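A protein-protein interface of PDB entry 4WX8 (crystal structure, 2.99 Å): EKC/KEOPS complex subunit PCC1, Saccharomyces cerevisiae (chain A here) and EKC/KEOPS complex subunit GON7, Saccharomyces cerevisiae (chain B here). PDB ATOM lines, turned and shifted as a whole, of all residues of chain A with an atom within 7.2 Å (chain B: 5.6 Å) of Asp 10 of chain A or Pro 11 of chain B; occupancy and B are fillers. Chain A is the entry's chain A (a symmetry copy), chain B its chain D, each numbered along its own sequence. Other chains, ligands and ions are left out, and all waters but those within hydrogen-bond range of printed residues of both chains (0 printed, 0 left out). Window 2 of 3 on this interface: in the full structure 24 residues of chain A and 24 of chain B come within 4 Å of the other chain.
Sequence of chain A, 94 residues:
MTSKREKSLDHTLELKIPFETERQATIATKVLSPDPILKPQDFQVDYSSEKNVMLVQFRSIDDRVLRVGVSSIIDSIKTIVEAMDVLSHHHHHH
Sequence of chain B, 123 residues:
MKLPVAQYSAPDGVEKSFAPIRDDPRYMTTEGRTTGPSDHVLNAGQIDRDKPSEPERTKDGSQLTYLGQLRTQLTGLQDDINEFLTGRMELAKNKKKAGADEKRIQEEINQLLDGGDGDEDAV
The backbone NH (N) of Ser 9 of chain B lies within hydrogen-bond range of the backbone carbonyl oxygen (O) of Thr 12 of chain A (2.7 Å).
The side-chain carboxylate (OD2) of Asp 63 of chain A lies within salt-bridge range of the guanidinium group (NH1) of Arg 88 of chain B, 3.1 Å away.
The backbone carbonyl oxygen (O) of Asp 10 of chain A lies close to the backbone carbonyl oxygen (O) of Ser 9 of chain B (3.3 Å).
Of the 7 printed residues of chain B, 4 touch a printed residue of chain A.
Of the 11 printed residues of chain A, 4 touch a printed residue of chain B.
Printed residues of chain A that touch a printed residue of chain B: Asp 10, His 11, Thr 12 and Asp 63.
Hydrophobic or aromatic side chains of chain A that line the printed part of chain B: His 11.
Among the printed residues, 7 pairs touch across the chains.
O of Asp 10 of chain A touches CA of Ala 10 of chain B, at 3.97 Å.
Asp 10 of chain A touches Pro 11 of chain B (OD2 to CB, 2.9 Å).
Ser 9 of chain B touches His 11 of chain A.
Pro 11 of chain B touches His 11 of chain A (CD to NE2, 3.3 Å).
Of chain B, only Ser 9 (3.3 Å), Ala 10 (3.97 Å) and Pro 11 (2.9 Å) come within 4 Å of Asp 10 of chain A.
Of the printed residues of chain B, His 11 of chain A touches Ser 9 and Pro 11.
Of the printed residues of chain B, Thr 12 of chain A touches Ser 9 (2.7 Å).
Of the printed residues of chain A, Ser 9 of chain B touches Asp 10 (3.3 Å), His 11 (3.5 Å) and Thr 12 (2.7 Å).
The nearest residue of chain A that does not touch Pro 11 of chain B is Ile 61 of chain A (6.0 Å).
The nearest printed residue of chain B that does not touch Asp 63 of chain A is Ala 10 of chain B (5.1 Å).
The backbone NH of Asp 10 of chain A sits at hydrogen-bond distance from the backbone carbonyl oxygen of Ser 60 of chain A, at 3.3 Å.
The backbone NH of Ser 60 of chain A lies within hydrogen-bond range of the backbone carbonyl oxygen of His 11 of chain A (3.0 Å).
OD1 of Asp 63 of chain A lies within hydrogen-bond range of ND1 of His 11 of chain A, at 2.5 Å.
OD2 of Asp 12 of chain B is in salt-bridge range of NH2 of Arg 88 of chain B, at 2.6 Å.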
ATOM      1  N   SER A   8      -3.760 -21.236   9.005  1.00  0.00           N
ATOM      2  CA  SER A   8      -3.343 -19.866   8.619  1.00  0.00           C
ATOM      3  C   SER A   8      -2.822 -19.093   9.807  1.00  0.00           C
ATOM      4  O   SER A   8      -3.257 -19.296  10.941  1.00  0.00           O
ATOM      5  CB  SER A   8      -4.476 -19.072   7.981  1.00  0.00           C
ATOM      6  OG  SER A   8      -3.915 -18.076   7.113  1.00  0.00           O
ATOM      7  N   LEU A   9      -1.868 -18.210   9.537  1.00  0.00           N
ATOM      8  CA  LEU A   9      -1.139 -17.557  10.595  1.00  0.00           C
ATOM      9  C   LEU A   9      -1.768 -16.206  10.819  1.00  0.00           C
ATOM     10  O   LEU A   9      -1.150 -15.190  10.539  1.00  0.00           O
ATOM     11  CB  LEU A   9       0.328 -17.394  10.192  1.00  0.00           C
ATOM     12  CG  LEU A   9       1.264 -18.611  10.163  1.00  0.00           C
ATOM     13  CD1 LEU A   9       2.606 -18.246   9.534  1.00  0.00           C
ATOM     14  CD2 LEU A   9       1.499 -19.171  11.569  1.00  0.00           C
ATOM     15  N   ASP A  10      -2.999 -16.180  11.310  1.00  0.00           N
ATOM     16  CA  ASP A  10      -3.742 -14.921  11.366  1.00  0.00           C
ATOM     17  C   ASP A  10      -3.832 -14.249  12.748  1.00  0.00           C
ATOM     18  O   ASP A  10      -4.545 -13.258  12.908  1.00  0.00           O
ATOM     19  CB  ASP A  10      -5.146 -15.129  10.810  1.00  0.00           C
ATOM     20  CG  ASP A  10      -5.893 -16.234  11.520  1.00  0.00           C
ATOM     21  OD1 ASP A  10      -5.353 -16.785  12.515  1.00  0.00           O
ATOM     22  OD2 ASP A  10      -7.024 -16.549  11.067  1.00  0.00           O
ATOM     23  N   HIS A  11      -3.127 -14.774  13.740  1.00  0.00           N
ATOM     24  CA  HIS A  11      -3.035 -14.097  15.020  1.00  0.00           C
ATOM     25  C   HIS A  11      -1.755 -13.298  15.007  1.00  0.00           C
ATOM     26  O   HIS A  11      -0.644 -13.848  15.040  1.00  0.00           O
ATOM     27  CB  HIS A  11      -3.025 -15.088  16.165  1.00  0.00           C
ATOM     28  CG  HIS A  11      -4.341 -15.779  16.380  1.00  0.00           C
ATOM     29  ND1 HIS A  11      -5.012 -15.745  17.584  1.00  0.00           N
ATOM     30  CD2 HIS A  11      -5.107 -16.519  15.544  1.00  0.00           C
ATOM     31  CE1 HIS A  11      -6.134 -16.433  17.478  1.00  0.00           C
ATOM     32  NE2 HIS A  11      -6.218 -16.908  16.249  1.00  0.00           N
ATOM     33  N   THR A  12      -1.915 -11.984  14.976  1.00  0.00           N
ATOM     34  CA  THR A  12      -0.871 -11.079  14.558  1.00  0.00           C
ATOM     35  C   THR A  12      -0.543 -10.099  15.646  1.00  0.00           C
ATOM     36  O   THR A  12      -1.442  -9.570  16.287  1.00  0.00           O
ATOM     37  CB  THR A  12      -1.388 -10.266  13.370  1.00  0.00           C
ATOM     38  OG1 THR A  12      -1.274 -11.071  12.191  1.00  0.00           O
ATOM     39  CG2 THR A  12      -0.609  -8.955  13.221  1.00  0.00           C
ATOM     40  N   LEU A  13       0.742  -9.824  15.829  1.00  0.00           N
ATOM     41  CA  LEU A  13       1.159  -8.792  16.745  1.00  0.00           C
ATOM     42  C   LEU A  13       2.421  -8.099  16.249  1.00  0.00           C
ATOM     43  O   LEU A  13       3.434  -8.747  16.010  1.00  0.00           O
ATOM     44  CB  LEU A  13       1.407  -9.401  18.099  1.00  0.00           C
ATOM     45  CG  LEU A  13       1.750  -8.358  19.144  1.00  0.00           C
ATOM     46  CD1 LEU A  13       1.116  -8.707  20.499  1.00  0.00           C
ATOM     47  CD2 LEU A  13       3.273  -8.277  19.239  1.00  0.00           C
ATOM     48  N   ARG A  59       3.624 -13.416  13.492  1.00  0.00           N
ATOM     49  CA  ARG A  59       2.458 -14.058  12.878  1.00  0.00           C
ATOM     50  C   ARG A  59       2.337 -15.464  13.469  1.00  0.00           C
ATOM     51  O   ARG A  59       3.361 -16.158  13.594  1.00  0.00           O
ATOM     52  CB  ARG A  59       2.625 -14.171  11.362  1.00  0.00           C
ATOM     53  CG  ARG A  59       2.741 -12.838  10.617  1.00  0.00           C
ATOM     54  CD  ARG A  59       2.931 -12.999   9.111  1.00  0.00           C
ATOM     55  NE  ARG A  59       4.296 -13.419   8.768  1.00  0.00           N
ATOM     56  CZ  ARG A  59       5.313 -12.583   8.531  1.00  0.00           C
ATOM     57  N   SER A  60       1.119 -15.910  13.813  1.00  0.00           N
ATOM     58  CA  SER A  60       0.945 -17.189  14.528  1.00  0.00           C
ATOM     59  C   SER A  60      -0.387 -17.918  14.346  1.00  0.00           C
ATOM     60  O   SER A  60      -1.390 -17.330  13.952  1.00  0.00           O
ATOM     61  CB  SER A  60       1.112 -16.935  16.010  1.00  0.00           C
ATOM     62  OG  SER A  60       0.742 -18.074  16.760  1.00  0.00           O
ATOM     63  N   ILE A  61      -0.386 -19.209  14.670  1.00  0.00           N
ATOM     64  CA  ILE A  61      -1.602 -20.061  14.572  1.00  0.00           C
ATOM     65  C   ILE A  61      -2.712 -19.535  15.470  1.00  0.00           C
ATOM     66  O   ILE A  61      -3.840 -19.305  15.014  1.00  0.00           O
ATOM     67  CB  ILE A  61      -1.343 -21.537  14.988  1.00  0.00           C
ATOM     68  N   ASP A  62      -2.358 -19.342  16.738  1.00  0.00           N
ATOM     69  CA  ASP A  62      -3.303 -18.971  17.772  1.00  0.00           C
ATOM     70  C   ASP A  62      -2.601 -18.176  18.865  1.00  0.00           C
ATOM     71  O   ASP A  62      -1.399 -17.949  18.800  1.00  0.00           O
ATOM     72  CB  ASP A  62      -3.891 -20.240  18.376  1.00  0.00           C
ATOM     73  CG  ASP A  62      -2.892 -20.986  19.248  1.00  0.00           C
ATOM     74  OD1 ASP A  62      -1.938 -20.321  19.735  1.00  0.00           O
ATOM     75  OD2 ASP A  62      -3.058 -22.225  19.447  1.00  0.00           O
ATOM     76  N   ASP A  63      -3.338 -17.795  19.892  1.00  0.00           N
ATOM     77  CA  ASP A  63      -2.787 -16.959  20.938  1.00  0.00           C
ATOM     78  C   ASP A  63      -1.730 -17.629  21.827  1.00  0.00           C
ATOM     79  O   ASP A  63      -0.840 -16.932  22.336  1.00  0.00           O
ATOM     80  CB  ASP A  63      -3.910 -16.381  21.788  1.00  0.00           C
ATOM     81  CG  ASP A  63      -4.811 -15.433  20.997  1.00  0.00           C
ATOM     82  OD1 ASP A  63      -4.415 -14.940  19.899  1.00  0.00           O
ATOM     83  OD2 ASP A  63      -5.927 -15.171  21.491  1.00  0.00           O
ATOM     84  N   SER B   9      -3.841  -8.262  16.287  1.00  0.00           N
ATOM     85  CA  SER B   9      -5.032  -8.614  15.513  1.00  0.00           C
ATOM     86  C   SER B   9      -5.350 -10.095  15.421  1.00  0.00           C
ATOM     87  O   SER B   9      -4.469 -10.920  15.218  1.00  0.00           O
ATOM     88  CB  SER B   9      -4.892  -8.104  14.122  1.00  0.00           C
ATOM     89  OG  SER B   9      -5.236  -6.752  14.155  1.00  0.00           O
ATOM     90  N   ALA B  10      -6.643 -10.411  15.522  1.00  0.00           N
ATOM     91  CA  ALA B  10      -7.095 -11.792  15.580  1.00  0.00           C
ATOM     92  C   ALA B  10      -8.264 -12.021  14.670  1.00  0.00           C
ATOM     93  O   ALA B  10      -9.102 -11.159  14.515  1.00  0.00           O
ATOM     94  CB  ALA B  10      -7.463 -12.148  16.993  1.00  0.00           C
ATOM     95  N   PRO B  11      -8.339 -13.221  14.090  1.00  0.00           N
ATOM     96  CA  PRO B  11      -9.246 -13.516  12.978  1.00  0.00           C
ATOM     97  C   PRO B  11     -10.701 -13.430  13.403  1.00  0.00           C
ATOM     98  O   PRO B  11     -11.593 -13.496  12.573  1.00  0.00           O
ATOM     99  CB  PRO B  11      -8.882 -14.951  12.601  1.00  0.00           C
ATOM    100  CG  PRO B  11      -8.382 -15.562  13.874  1.00  0.00           C
ATOM    101  CD  PRO B  11      -7.774 -14.449  14.687  1.00  0.00           C
ATOM    102  N   ASP B  12     -10.940 -13.277  14.691  1.00  0.00           N
ATOM    103  CA  ASP B  12     -12.289 -13.141  15.167  1.00  0.00           C
ATOM    104  C   ASP B  12     -12.667 -11.696  15.447  1.00  0.00           C
ATOM    105  O   ASP B  12     -13.354 -11.425  16.411  1.00  0.00           O
ATOM    106  CB  ASP B  12     -12.416 -13.891  16.461  1.00  0.00           C
ATOM    107  CG  ASP B  12     -11.581 -13.294  17.521  1.00  0.00           C
ATOM    108  OD1 ASP B  12     -10.371 -13.138  17.286  1.00  0.00           O
ATOM    109  OD2 ASP B  12     -12.133 -12.962  18.578  1.00  0.00           O
ATOM    110  N   GLY B  13     -12.211 -10.763  14.625  1.00  0.00           N
ATOM    111  CA  GLY B  13     -12.696  -9.396  14.708  1.00  0.00           C
ATOM    112  C   GLY B  13     -12.182  -8.596  15.880  1.00  0.00           C
ATOM    113  O   GLY B  13     -12.678  -7.509  16.115  1.00  0.00           O
ATOM    114  N   VAL B  14     -11.204  -9.111  16.623  1.00  0.00           N
ATOM    115  CA  VAL B  14     -10.611  -8.338  17.743  1.00  0.00           C
ATOM    116  C   VAL B  14      -9.302  -7.617  17.403  1.00  0.00           C
ATOM    117  O   VAL B  14      -8.413  -8.198  16.791  1.00  0.00           O
ATOM    118  CB  VAL B  14     -10.368  -9.236  18.980  1.00  0.00           C
ATOM    119  CG1 VAL B  14      -9.475  -8.557  20.006  1.00  0.00           C
ATOM    120  CG2 VAL B  14     -11.695  -9.563  19.628  1.00  0.00           C
ATOM    121  N   ARG B  88      -7.058 -14.511  26.709  1.00  0.00           N
ATOM    122  CA  ARG B  88      -7.778 -14.898  25.536  1.00  0.00           C
ATOM    123  C   ARG B  88      -7.815 -16.387  25.426  1.00  0.00           C
ATOM    124  O   ARG B  88      -8.830 -16.950  25.048  1.00  0.00           O
ATOM    125  CB  ARG B  88      -7.158 -14.292  24.311  1.00  0.00           C
ATOM    126  CG  ARG B  88      -7.516 -12.828  24.168  1.00  0.00           C
ATOM    127  CD  ARG B  88      -7.503 -12.470  22.712  1.00  0.00           C
ATOM    128  NE  ARG B  88      -8.819 -12.506  22.106  1.00  0.00           N
ATOM    129  CZ  ARG B  88      -9.051 -12.897  20.858  1.00  0.00           C
ATOM    130  NH1 ARG B  88      -8.077 -13.346  20.104  1.00  0.00           N
ATOM    131  NH2 ARG B  88     -10.270 -12.875  20.359  1.00  0.00           N
